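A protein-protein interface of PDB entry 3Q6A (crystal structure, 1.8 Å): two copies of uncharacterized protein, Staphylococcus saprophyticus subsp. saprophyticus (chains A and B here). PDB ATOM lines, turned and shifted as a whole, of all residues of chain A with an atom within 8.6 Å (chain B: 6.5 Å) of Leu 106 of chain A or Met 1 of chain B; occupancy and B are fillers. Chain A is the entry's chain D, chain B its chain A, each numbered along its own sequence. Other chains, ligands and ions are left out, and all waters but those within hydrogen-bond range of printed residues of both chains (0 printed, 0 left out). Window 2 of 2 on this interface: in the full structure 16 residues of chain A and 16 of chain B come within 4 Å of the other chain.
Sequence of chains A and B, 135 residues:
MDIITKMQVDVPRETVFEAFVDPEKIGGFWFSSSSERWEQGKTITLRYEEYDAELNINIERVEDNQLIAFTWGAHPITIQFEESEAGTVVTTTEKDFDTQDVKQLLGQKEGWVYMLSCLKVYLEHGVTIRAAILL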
ATOM      1  N   ILE A   3     -17.576   9.989 -15.879  1.00  0.00           N
ATOM      2  CA  ILE A   3     -16.177   9.692 -16.132  1.00  0.00           C
ATOM      3  C   ILE A   3     -15.884   8.327 -15.529  1.00  0.00           C
ATOM      4  O   ILE A   3     -15.822   8.171 -14.312  1.00  0.00           O
ATOM      5  CB  ILE A   3     -15.256  10.752 -15.498  1.00  0.00           C
ATOM      6  CG1 ILE A   3     -15.691  12.146 -15.958  1.00  0.00           C
ATOM      7  CG2 ILE A   3     -13.812  10.491 -15.888  1.00  0.00           C
ATOM      8  CD1 ILE A   3     -14.890  13.278 -15.345  1.00  0.00           C
ATOM      9  N   PHE A  97     -21.779  15.030 -15.432  1.00  0.00           N
ATOM     10  CA  PHE A  97     -20.962  16.095 -16.009  1.00  0.00           C
ATOM     11  C   PHE A  97     -21.575  16.537 -17.332  1.00  0.00           C
ATOM     12  O   PHE A  97     -22.356  15.800 -17.933  1.00  0.00           O
ATOM     13  CB  PHE A  97     -19.538  15.599 -16.261  1.00  0.00           C
ATOM     14  CG  PHE A  97     -18.721  15.440 -15.015  1.00  0.00           C
ATOM     15  CD1 PHE A  97     -18.046  16.523 -14.473  1.00  0.00           C
ATOM     16  CD2 PHE A  97     -18.619  14.207 -14.387  1.00  0.00           C
ATOM     17  CE1 PHE A  97     -17.278  16.384 -13.327  1.00  0.00           C
ATOM     18  CE2 PHE A  97     -17.854  14.056 -13.239  1.00  0.00           C
ATOM     19  CZ  PHE A  97     -17.180  15.148 -12.705  1.00  0.00           C
ATOM     20  N   ASP A  98     -21.211  17.733 -17.785  1.00  0.00           N
ATOM     21  CA  ASP A  98     -21.723  18.270 -19.042  1.00  0.00           C
ATOM     22  C   ASP A  98     -20.605  18.360 -20.077  1.00  0.00           C
ATOM     23  O   ASP A  98     -19.424  18.336 -19.730  1.00  0.00           O
ATOM     24  CB  ASP A  98     -22.336  19.658 -18.812  1.00  0.00           C
ATOM     25  N   ASP A 101     -18.142  21.831 -20.596  1.00  0.00           N
ATOM     26  CA  ASP A 101     -16.825  21.957 -19.981  1.00  0.00           C
ATOM     27  C   ASP A 101     -15.921  20.767 -20.285  1.00  0.00           C
ATOM     28  O   ASP A 101     -15.815  19.832 -19.484  1.00  0.00           O
ATOM     29  CB  ASP A 101     -16.969  22.139 -18.464  1.00  0.00           C
ATOM     30  N   VAL A 102     -15.274  20.808 -21.447  1.00  0.00           N
ATOM     31  CA  VAL A 102     -14.358  19.754 -21.852  1.00  0.00           C
ATOM     32  C   VAL A 102     -13.126  19.843 -20.950  1.00  0.00           C
ATOM     33  O   VAL A 102     -12.520  18.830 -20.587  1.00  0.00           O
ATOM     34  CB  VAL A 102     -13.958  19.940 -23.319  1.00  0.00           C
ATOM     35  N   LYS A 103     -12.770  21.068 -20.581  1.00  0.00           N
ATOM     36  CA  LYS A 103     -11.618  21.302 -19.718  1.00  0.00           C
ATOM     37  C   LYS A 103     -11.787  20.593 -18.376  1.00  0.00           C
ATOM     38  O   LYS A 103     -10.871  19.925 -17.905  1.00  0.00           O
ATOM     39  CB  LYS A 103     -11.421  22.806 -19.499  1.00  0.00           C
ATOM     40  N   GLN A 104     -12.964  20.724 -17.767  1.00  0.00           N
ATOM     41  CA  GLN A 104     -13.218  20.078 -16.486  1.00  0.00           C
ATOM     42  C   GLN A 104     -13.149  18.556 -16.588  1.00  0.00           C
ATOM     43  O   GLN A 104     -12.594  17.896 -15.700  1.00  0.00           O
ATOM     44  CB  GLN A 104     -14.586  20.494 -15.938  1.00  0.00           C
ATOM     45  CG  GLN A 104     -15.074  19.641 -14.780  1.00  0.00           C
ATOM     46  CD  GLN A 104     -16.375  20.160 -14.174  1.00  0.00           C
ATOM     47  OE1 GLN A 104     -17.281  20.595 -14.891  1.00  0.00           O
ATOM     48  NE2 GLN A 104     -16.472  20.102 -12.848  1.00  0.00           N
ATOM     49  N   LEU A 105     -13.737  18.017 -17.655  1.00  0.00           N
ATOM     50  CA  LEU A 105     -13.747  16.579 -17.910  1.00  0.00           C
ATOM     51  C   LEU A 105     -12.325  16.054 -18.021  1.00  0.00           C
ATOM     52  O   LEU A 105     -11.978  15.050 -17.396  1.00  0.00           O
ATOM     53  CB  LEU A 105     -14.487  16.253 -19.221  1.00  0.00           C
ATOM     54  CG  LEU A 105     -16.006  16.451 -19.263  1.00  0.00           C
ATOM     55  CD1 LEU A 105     -16.532  16.057 -20.630  1.00  0.00           C
ATOM     56  CD2 LEU A 105     -16.669  15.607 -18.196  1.00  0.00           C
ATOM     57  N   LEU A 106     -11.502  16.724 -18.830  1.00  0.00           N
ATOM     58  CA  LEU A 106     -10.126  16.274 -19.023  1.00  0.00           C
ATOM     59  C   LEU A 106      -9.343  16.291 -17.725  1.00  0.00           C
ATOM     60  O   LEU A 106      -8.562  15.381 -17.451  1.00  0.00           O
ATOM     61  CB  LEU A 106      -9.419  17.136 -20.077  1.00  0.00           C
ATOM     62  CG  LEU A 106      -9.893  16.973 -21.528  1.00  0.00           C
ATOM     63  CD1 LEU A 106      -9.362  18.111 -22.395  1.00  0.00           C
ATOM     64  CD2 LEU A 106      -9.415  15.645 -22.057  1.00  0.00           C
ATOM     65  N   GLY A 107      -9.552  17.332 -16.929  1.00  0.00           N
ATOM     66  CA  GLY A 107      -8.849  17.444 -15.671  1.00  0.00           C
ATOM     67  C   GLY A 107      -9.231  16.347 -14.698  1.00  0.00           C
ATOM     68  O   GLY A 107      -8.373  15.799 -14.015  1.00  0.00           O
ATOM     69  N   GLN A 108     -10.513  16.026 -14.613  1.00  0.00           N
ATOM     70  CA  GLN A 108     -10.936  14.980 -13.694  1.00  0.00           C
ATOM     71  C   GLN A 108     -10.446  13.622 -14.189  1.00  0.00           C
ATOM     72  O   GLN A 108      -9.977  12.806 -13.403  1.00  0.00           O
ATOM     73  CB  GLN A 108     -12.454  14.978 -13.540  1.00  0.00           C
ATOM     74  CG  GLN A 108     -12.953  16.133 -12.680  1.00  0.00           C
ATOM     75  CD  GLN A 108     -12.455  16.044 -11.248  1.00  0.00           C
ATOM     76  OE1 GLN A 108     -13.029  15.333 -10.419  1.00  0.00           O
ATOM     77  NE2 GLN A 108     -11.369  16.753 -10.954  1.00  0.00           N
ATOM     78  N   LYS A 109     -10.559  13.391 -15.491  1.00  0.00           N
ATOM     79  CA  LYS A 109     -10.081  12.133 -16.073  1.00  0.00           C
ATOM     80  C   LYS A 109      -8.608  11.940 -15.683  1.00  0.00           C
ATOM     81  O   LYS A 109      -8.188  10.852 -15.267  1.00  0.00           O
ATOM     82  CB  LYS A 109     -10.223  12.176 -17.595  1.00  0.00           C
ATOM     83  CG  LYS A 109      -9.852  10.855 -18.280  1.00  0.00           C
ATOM     84  CD  LYS A 109     -10.844   9.729 -17.910  1.00  0.00           C
ATOM     85  CE  LYS A 109     -10.427   8.414 -18.598  1.00  0.00           C
ATOM     86  NZ  LYS A 109     -11.371   7.310 -18.245  1.00  0.00           N
ATOM     87  N   GLU A 110      -7.827  13.001 -15.828  1.00  0.00           N
ATOM     88  CA  GLU A 110      -6.414  12.970 -15.484  1.00  0.00           C
ATOM     89  C   GLU A 110      -6.244  12.540 -14.027  1.00  0.00           C
ATOM     90  O   GLU A 110      -5.430  11.683 -13.718  1.00  0.00           O
ATOM     91  CB  GLU A 110      -5.813  14.361 -15.678  1.00  0.00           C
ATOM     92  CG  GLU A 110      -4.368  14.479 -15.265  1.00  0.00           C
ATOM     93  CD  GLU A 110      -3.849  15.850 -15.557  1.00  0.00           C
ATOM     94  OE1 GLU A 110      -4.358  16.805 -14.935  1.00  0.00           O
ATOM     95  OE2 GLU A 110      -2.959  15.976 -16.409  1.00  0.00           O
ATOM     96  N   GLY A 111      -7.019  13.137 -13.129  1.00  0.00           N
ATOM     97  CA  GLY A 111      -6.885  12.783 -11.724  1.00  0.00           C
ATOM     98  C   GLY A 111      -7.142  11.308 -11.443  1.00  0.00           C
ATOM     99  O   GLY A 111      -6.401  10.669 -10.685  1.00  0.00           O
ATOM    100  N   TRP A 112      -8.192  10.775 -12.049  1.00  0.00           N
ATOM    101  CA  TRP A 112      -8.563   9.375 -11.854  1.00  0.00           C
ATOM    102  C   TRP A 112      -7.521   8.450 -12.437  1.00  0.00           C
ATOM    103  O   TRP A 112      -7.133   7.479 -11.794  1.00  0.00           O
ATOM    104  CB  TRP A 112      -9.921   9.085 -12.491  1.00  0.00           C
ATOM    105  CG  TRP A 112     -11.069   9.670 -11.721  1.00  0.00           C
ATOM    106  CD1 TRP A 112     -11.899  10.686 -12.120  1.00  0.00           C
ATOM    107  CD2 TRP A 112     -11.482   9.308 -10.395  1.00  0.00           C
ATOM    108  NE1 TRP A 112     -12.800  10.983 -11.117  1.00  0.00           N
ATOM    109  CE2 TRP A 112     -12.565  10.152 -10.049  1.00  0.00           C
ATOM    110  CE3 TRP A 112     -11.039   8.352  -9.462  1.00  0.00           C
ATOM    111  CZ2 TRP A 112     -13.211  10.067  -8.812  1.00  0.00           C
ATOM    112  CZ3 TRP A 112     -11.682   8.272  -8.232  1.00  0.00           C
ATOM    113  CH2 TRP A 112     -12.757   9.125  -7.919  1.00  0.00           C
ATOM    114  N   VAL A 113      -7.041   8.765 -13.641  1.00  0.00           N
ATOM    115  CA  VAL A 113      -6.029   7.911 -14.262  1.00  0.00           C
ATOM    116  C   VAL A 113      -4.745   7.929 -13.458  1.00  0.00           C
ATOM    117  O   VAL A 113      -4.141   6.896 -13.233  1.00  0.00           O
ATOM    118  CB  VAL A 113      -5.707   8.356 -15.696  1.00  0.00           C
ATOM    119  CG1 VAL A 113      -4.618   7.454 -16.285  1.00  0.00           C
ATOM    120  CG2 VAL A 113      -6.981   8.285 -16.551  1.00  0.00           C
ATOM    121  N   LEU A 134      -6.548  14.651  -6.673  1.00  0.00           N
ATOM    122  CA  LEU A 134      -7.783  14.443  -7.430  1.00  0.00           C
ATOM    123  C   LEU A 134      -8.950  15.300  -6.922  1.00  0.00           C
ATOM    124  O   LEU A 134      -9.390  16.240  -7.599  1.00  0.00           O
ATOM    125  CB  LEU A 134      -8.162  12.956  -7.400  1.00  0.00           C
ATOM    126  CG  LEU A 134      -9.473  12.515  -8.063  1.00  0.00           C
ATOM    127  CD1 LEU A 134      -9.564  13.019  -9.491  1.00  0.00           C
ATOM    128  CD2 LEU A 134      -9.540  11.006  -8.032  1.00  0.00           C
ATOM    129  N   MET B   1      -8.634  21.779 -30.761  1.00  0.00           N
ATOM    130  CA  MET B   1      -8.265  21.630 -29.320  1.00  0.00           C
ATOM    131  C   MET B   1      -7.071  20.700 -29.148  1.00  0.00           C
ATOM    132  O   MET B   1      -6.971  19.667 -29.830  1.00  0.00           O
ATOM    133  CB  MET B   1      -9.427  21.057 -28.523  1.00  0.00           C
ATOM    134  CG  MET B   1      -9.522  21.647 -27.133  1.00  0.00           C
ATOM    135  SD  MET B   1     -10.133  20.404 -25.801  1.00  0.00           S
ATOM    136  CE  MET B   1      -8.693  20.661 -24.540  1.00  0.00           C
ATOM    137  N   ASP B   2      -6.173  21.055 -28.232  1.00  0.00           N
ATOM    138  CA  ASP B   2      -4.986  20.229 -27.977  1.00  0.00           C
ATOM    139  C   ASP B   2      -5.065  19.537 -26.601  1.00  0.00           C
ATOM    140  O   ASP B   2      -5.572  20.110 -25.635  1.00  0.00           O
ATOM    141  CB  ASP B   2      -3.706  21.074 -28.016  1.00  0.00           C
ATOM    142  CG  ASP B   2      -3.478  21.765 -29.353  1.00  0.00           C
ATOM    143  OD1 ASP B   2      -4.084  21.373 -30.377  1.00  0.00           O
ATOM    144  OD2 ASP B   2      -2.658  22.711 -29.369  1.00  0.00           O
ATOM    145  N   ILE B   3      -4.554  18.313 -26.523  1.00  0.00           N
ATOM    146  CA  ILE B   3      -4.567  17.550 -25.277  1.00  0.00           C
ATOM    147  C   ILE B   3      -3.163  17.697 -24.715  1.00  0.00           C
ATOM    148  O   ILE B   3      -2.218  17.120 -25.238  1.00  0.00           O
ATOM    149  CB  ILE B   3      -4.873  16.066 -25.550  1.00  0.00           C
ATOM    150  CG1 ILE B   3      -6.223  15.973 -26.295  1.00  0.00           C
ATOM    151  CG2 ILE B   3      -4.937  15.277 -24.231  1.00  0.00           C
ATOM    152  CD1 ILE B   3      -6.696  14.543 -26.535  1.00  0.00           C
ATOM    153  N   ILE B   4      -3.054  18.480 -23.655  1.00  0.00           N
ATOM    154  CA  ILE B   4      -1.766  18.784 -23.028  1.00  0.00           C
ATOM    155  C   ILE B   4      -1.672  18.128 -21.677  1.00  0.00           C
ATOM    156  O   ILE B   4      -2.579  18.274 -20.848  1.00  0.00           O
ATOM    157  CB  ILE B   4      -1.623  20.317 -22.846  1.00  0.00           C
ATOM    158  CG1 ILE B   4      -1.787  21.015 -24.200  1.00  0.00           C
ATOM    159  CG2 ILE B   4      -0.239  20.662 -22.279  1.00  0.00           C
ATOM    160  CD1 ILE B   4      -2.104  22.502 -24.088  1.00  0.00           C
ATOM    161  N   HIS B  75      -2.866  14.171 -36.230  1.00  0.00           N
ATOM    162  CA  HIS B  75      -2.599  14.827 -34.955  1.00  0.00           C
ATOM    163  C   HIS B  75      -1.112  15.046 -34.655  1.00  0.00           C
ATOM    164  O   HIS B  75      -0.413  14.125 -34.253  1.00  0.00           O
ATOM    165  CB  HIS B  75      -3.218  14.018 -33.805  1.00  0.00           C
ATOM    166  CG  HIS B  75      -4.696  13.810 -33.935  1.00  0.00           C
ATOM    167  ND1 HIS B  75      -5.601  14.848 -33.889  1.00  0.00           N
ATOM    168  CD2 HIS B  75      -5.423  12.689 -34.150  1.00  0.00           C
ATOM    169  CE1 HIS B  75      -6.821  14.375 -34.074  1.00  0.00           C
ATOM    170  NE2 HIS B  75      -6.740  13.067 -34.235  1.00  0.00           N
ATOM    171  N   GLU B  94      -0.864  16.613 -27.900  1.00  0.00           N
ATOM    172  CA  GLU B  94      -1.367  15.928 -29.101  1.00  0.00           C
ATOM    173  C   GLU B  94      -2.386  16.953 -29.593  1.00  0.00           C
ATOM    174  O   GLU B  94      -3.340  17.289 -28.891  1.00  0.00           O
ATOM    175  CB  GLU B  94      -2.048  14.596 -28.771  1.00  0.00           C
ATOM    176  CG  GLU B  94      -2.405  13.807 -30.039  1.00  0.00           C
ATOM    177  CD  GLU B  94      -3.003  12.431 -29.774  1.00  0.00           C
ATOM    178  OE1 GLU B  94      -3.264  12.081 -28.596  1.00  0.00           O
ATOM    179  OE2 GLU B  94      -3.222  11.704 -30.769  1.00  0.00           O
ATOM    180  N   LYS B  95      -2.170  17.426 -30.812  1.00  0.00           N
ATOM    181  CA  LYS B  95      -2.963  18.508 -31.366  1.00  0.00           C
ATOM    182  C   LYS B  95      -4.076  18.224 -32.366  1.00  0.00           C
ATOM    183  O   LYS B  95      -4.142  17.159 -32.974  1.00  0.00           O
ATOM    184  CB  LYS B  95      -2.000  19.519 -31.992  1.00  0.00           C
ATOM    185  CG  LYS B  95      -0.847  19.897 -31.064  1.00  0.00           C
ATOM    186  CD  LYS B  95       0.229  20.686 -31.793  1.00  0.00           C
ATOM    187  CE  LYS B  95       1.367  21.067 -30.835  1.00  0.00           C
ATOM    188  NZ  LYS B  95       2.428  21.924 -31.465  1.00  0.00           N
ATOM    189  N   ASP B  96      -4.936  19.228 -32.480  1.00  0.00           N
ATOM    190  CA  ASP B  96      -6.035  19.276 -33.429  1.00  0.00           C
ATOM    191  C   ASP B  96      -7.166  18.270 -33.321  1.00  0.00           C
ATOM    192  O   ASP B  96      -7.411  17.480 -34.236  1.00  0.00           O
ATOM    193  CB  ASP B  96      -5.442  19.273 -34.840  1.00  0.00           C
ATOM    194  CG  ASP B  96      -4.423  20.380 -35.040  1.00  0.00           C
ATOM    195  OD1 ASP B  96      -4.651  21.502 -34.534  1.00  0.00           O
ATOM    196  OD2 ASP B  96      -3.399  20.136 -35.702  1.00  0.00           O
ATOM    197  N   PHE B  97      -7.874  18.336 -32.200  1.00  0.00           N
ATOM    198  CA  PHE B  97      -9.019  17.475 -31.942  1.00  0.00           C
ATOM    199  C   PHE B  97     -10.282  18.311 -32.000  1.00  0.00           C
ATOM    200  O   PHE B  97     -10.239  19.509 -31.742  1.00  0.00           O
ATOM    201  CB  PHE B  97      -8.915  16.877 -30.548  1.00  0.00           C
ATOM    202  CG  PHE B  97      -7.913  15.781 -30.445  1.00  0.00           C
ATOM    203  CD1 PHE B  97      -8.241  14.494 -30.843  1.00  0.00           C
ATOM    204  CD2 PHE B  97      -6.629  16.038 -29.965  1.00  0.00           C
ATOM    205  CE1 PHE B  97      -7.319  13.471 -30.775  1.00  0.00           C
ATOM    206  CE2 PHE B  97      -5.686  15.008 -29.891  1.00  0.00           C
ATOM    207  CZ  PHE B  97      -6.031  13.728 -30.292  1.00  0.00           C
ATOM    208  N   ASP B  98     -11.403  17.677 -32.335  1.00  0.00           N
ATOM    209  CA  ASP B  98     -12.680  18.373 -32.377  1.00  0.00           C
ATOM    210  C   ASP B  98     -13.270  18.234 -30.977  1.00  0.00           C
ATOM    211  O   ASP B  98     -12.991  17.267 -30.272  1.00  0.00           O
ATOM    212  CB  ASP B  98     -13.602  17.728 -33.401  1.00  0.00           C
ATOM    213  N   THR B  99     -14.071  19.206 -30.566  1.00  0.00           N
ATOM    214  CA  THR B  99     -14.691  19.154 -29.249  1.00  0.00           C
ATOM    215  C   THR B  99     -16.013  18.398 -29.342  1.00  0.00           C
ATOM    216  O   THR B  99     -16.924  18.605 -28.542  1.00  0.00           O
ATOM    217  CB  THR B  99     -14.928  20.578 -28.699  1.00  0.00           C
ATOM    218  OG1 THR B  99     -15.552  21.383 -29.705  1.00  0.00           O
ATOM    219  CG2 THR B  99     -13.610  21.218 -28.301  1.00  0.00           C
ATOM    220  N   VAL B 102     -16.110  13.592 -27.249  1.00  0.00           N
ATOM    221  CA  VAL B 102     -15.555  13.788 -25.918  1.00  0.00           C
ATOM    222  C   VAL B 102     -14.885  12.483 -25.498  1.00  0.00           C
ATOM    223  O   VAL B 102     -13.886  12.487 -24.775  1.00  0.00           O
ATOM    224  CB  VAL B 102     -16.666  14.153 -24.934  1.00  0.00           C
ATOM    225  N   LEU B 105     -11.370  12.448 -26.835  1.00  0.00           N
ATOM    226  CA  LEU B 105     -10.496  13.322 -26.056  1.00  0.00           C
ATOM    227  C   LEU B 105     -10.151  12.668 -24.715  1.00  0.00           C
ATOM    228  O   LEU B 105      -8.995  12.701 -24.268  1.00  0.00           O
ATOM    229  CB  LEU B 105     -11.171  14.683 -25.803  1.00  0.00           C
ATOM    230  CG  LEU B 105     -11.211  15.653 -26.988  1.00  0.00           C
ATOM    231  CD1 LEU B 105     -12.305  16.685 -26.791  1.00  0.00           C
ATOM    232  CD2 LEU B 105      -9.843  16.321 -27.134  1.00  0.00           C
ATOM    233  N   LEU B 106     -11.154  12.072 -24.083  1.00  0.00           N
ATOM    234  CA  LEU B 106     -10.974  11.432 -22.790  1.00  0.00           C
ATOM    235  C   LEU B 106     -10.090  10.194 -22.910  1.00  0.00           C
ATOM    236  O   LEU B 106      -9.280   9.913 -22.024  1.00  0.00           O
ATOM    237  CB  LEU B 106     -12.344  11.075 -22.208  1.00  0.00           C
ATOM    238  CG  LEU B 106     -12.720  11.585 -20.810  1.00  0.00           C
ATOM    239  CD1 LEU B 106     -12.227  12.992 -20.593  1.00  0.00           C
ATOM    240  CD2 LEU B 106     -14.233  11.528 -20.648  1.00  0.00           C
ATOM    241  N   LYS B 109      -6.500  11.405 -23.527  1.00  0.00           N
ATOM    242  CA  LYS B 109      -5.972  12.008 -22.308  1.00  0.00           C
ATOM    243  C   LYS B 109      -5.498  10.893 -21.376  1.00  0.00           C
ATOM    244  O   LYS B 109      -4.403  10.957 -20.787  1.00  0.00           O
ATOM    245  CB  LYS B 109      -7.062  12.825 -21.621  1.00  0.00           C
ATOM    246  CG  LYS B 109      -6.605  13.436 -20.314  1.00  0.00           C
ATOM    247  CD  LYS B 109      -5.508  14.470 -20.562  1.00  0.00           C
ATOM    248  CE  LYS B 109      -5.165  15.194 -19.262  1.00  0.00           C
ATOM    249  NZ  LYS B 109      -4.215  16.315 -19.571  1.00  0.00           N
ATOM    250  N   VAL B 113      -1.695  10.356 -19.857  1.00  0.00           N
ATOM    251  CA  VAL B 113      -1.472  10.344 -18.409  1.00  0.00           C
ATOM    252  C   VAL B 113      -0.869   9.021 -17.956  1.00  0.00           C
ATOM    253  O   VAL B 113       0.072   8.993 -17.135  1.00  0.00           O
ATOM    254  CB  VAL B 113      -2.779  10.627 -17.648  1.00  0.00           C
ATOM    255  CG1 VAL B 113      -2.542  10.468 -16.138  1.00  0.00           C
ATOM    256  CG2 VAL B 113      -3.264  12.035 -17.955  1.00  0.00           C
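Leu 105 of chain A touches Leu 106 of chain B, and with the chains exchanged Leu 106 of chain A touches Leu 105 of chain B.
Leu 106 of chain A touches Lys 109 of chain B, and with the chains exchanged Lys 109 of chain A touches Leu 106 of chain B.
Val 113 of chain B touches its own counterpart, Val 113 of chain A.
Of the 17 printed residues of chain A, 5 touch a printed residue of chain B.
Of the 16 printed residues of chain B, 5 touch a printed residue of chain A.
Hydrophobic or aromatic side chains of chain B within 4 Å of the printed part of chain A: Met 1, Leu 106 and Val 113.
Among the printed residues, Asp or Glu carboxylates within 4 Å of a Lys or Arg side-chain nitrogen of the other chain: Glu 110 of chain A with Lys 109 of chain B (3.4 Å).
N of Phe 97 of chain B sits at hydrogen-bond distance from O of Met 1 of chain B, 2.9 Å away.
The backbone NH of Asp 96 of chain B is in hydrogen-bond range of the backbone carbonyl oxygen of Met 1 of chain B, at 3.4 Å.
The backbone carbonyl oxygen (O) of Ile 4 of chain B lies within hydrogen-bond range of the side-chain amino group (NZ) of Lys 109 of chain B (2.9 Å).
Lys 103 of chain A touches none of the printed residues of chain B.
Of chain B, only Met 1, Leu 105 and Lys 109 come within 4 Å of Leu 106 of chain A.
Gly 107 of chain A touches none of the printed residues of chain B.
Printed residues of chain B within 4 Å of Glu 110 of chain A: Lys 109 (3.4 Å) and Val 113 (3.8 Å).
Printed residues of chain B within 4 Å of Val 113 of chain A: Val 113.
Met 1 of chain B touches one residue of chain A.
Of the printed residues of chain A, Leu 105 of chain B touches Leu 106 (3.7 Å).
Printed residues of chain A within 4 Å of Val 113 of chain B: Glu 110 (3.8 Å) and Val 113 (3.7 Å).
The nearest residue of chain B that does not touch Leu 106 of chain A is Leu 106 of chain B (4.1 Å).
The nearest residue of chain A that does not touch Met 1 of chain B is Val 102 of chain A (4.6 Å).
O of Leu 105 of chain A touches CD1 of Leu 106 of chain B, at 3.8 Å.
Leu 106 of chain A touches Met 1 of chain B.
O of Leu 105 of chain B touches CD2 of Leu 106 of chain A (3.7 Å).
CD2 of Leu 106 of chain A touches CB of Lys 109 of chain B, at 3.7 Å.
Lys 109 of chain A touches Leu 106 of chain B.
Val 113 of chain B touches Glu 110 of chain A (CG2 to CG, 3.8 Å).
Val 113 of chain A touches Val 113 of chain B (CG1 to CG1, 3.7 Å).
NZ of Lys 109 of chain B is in salt-bridge range of OE2 of Glu 110 of chain A, 3.4 Å away.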
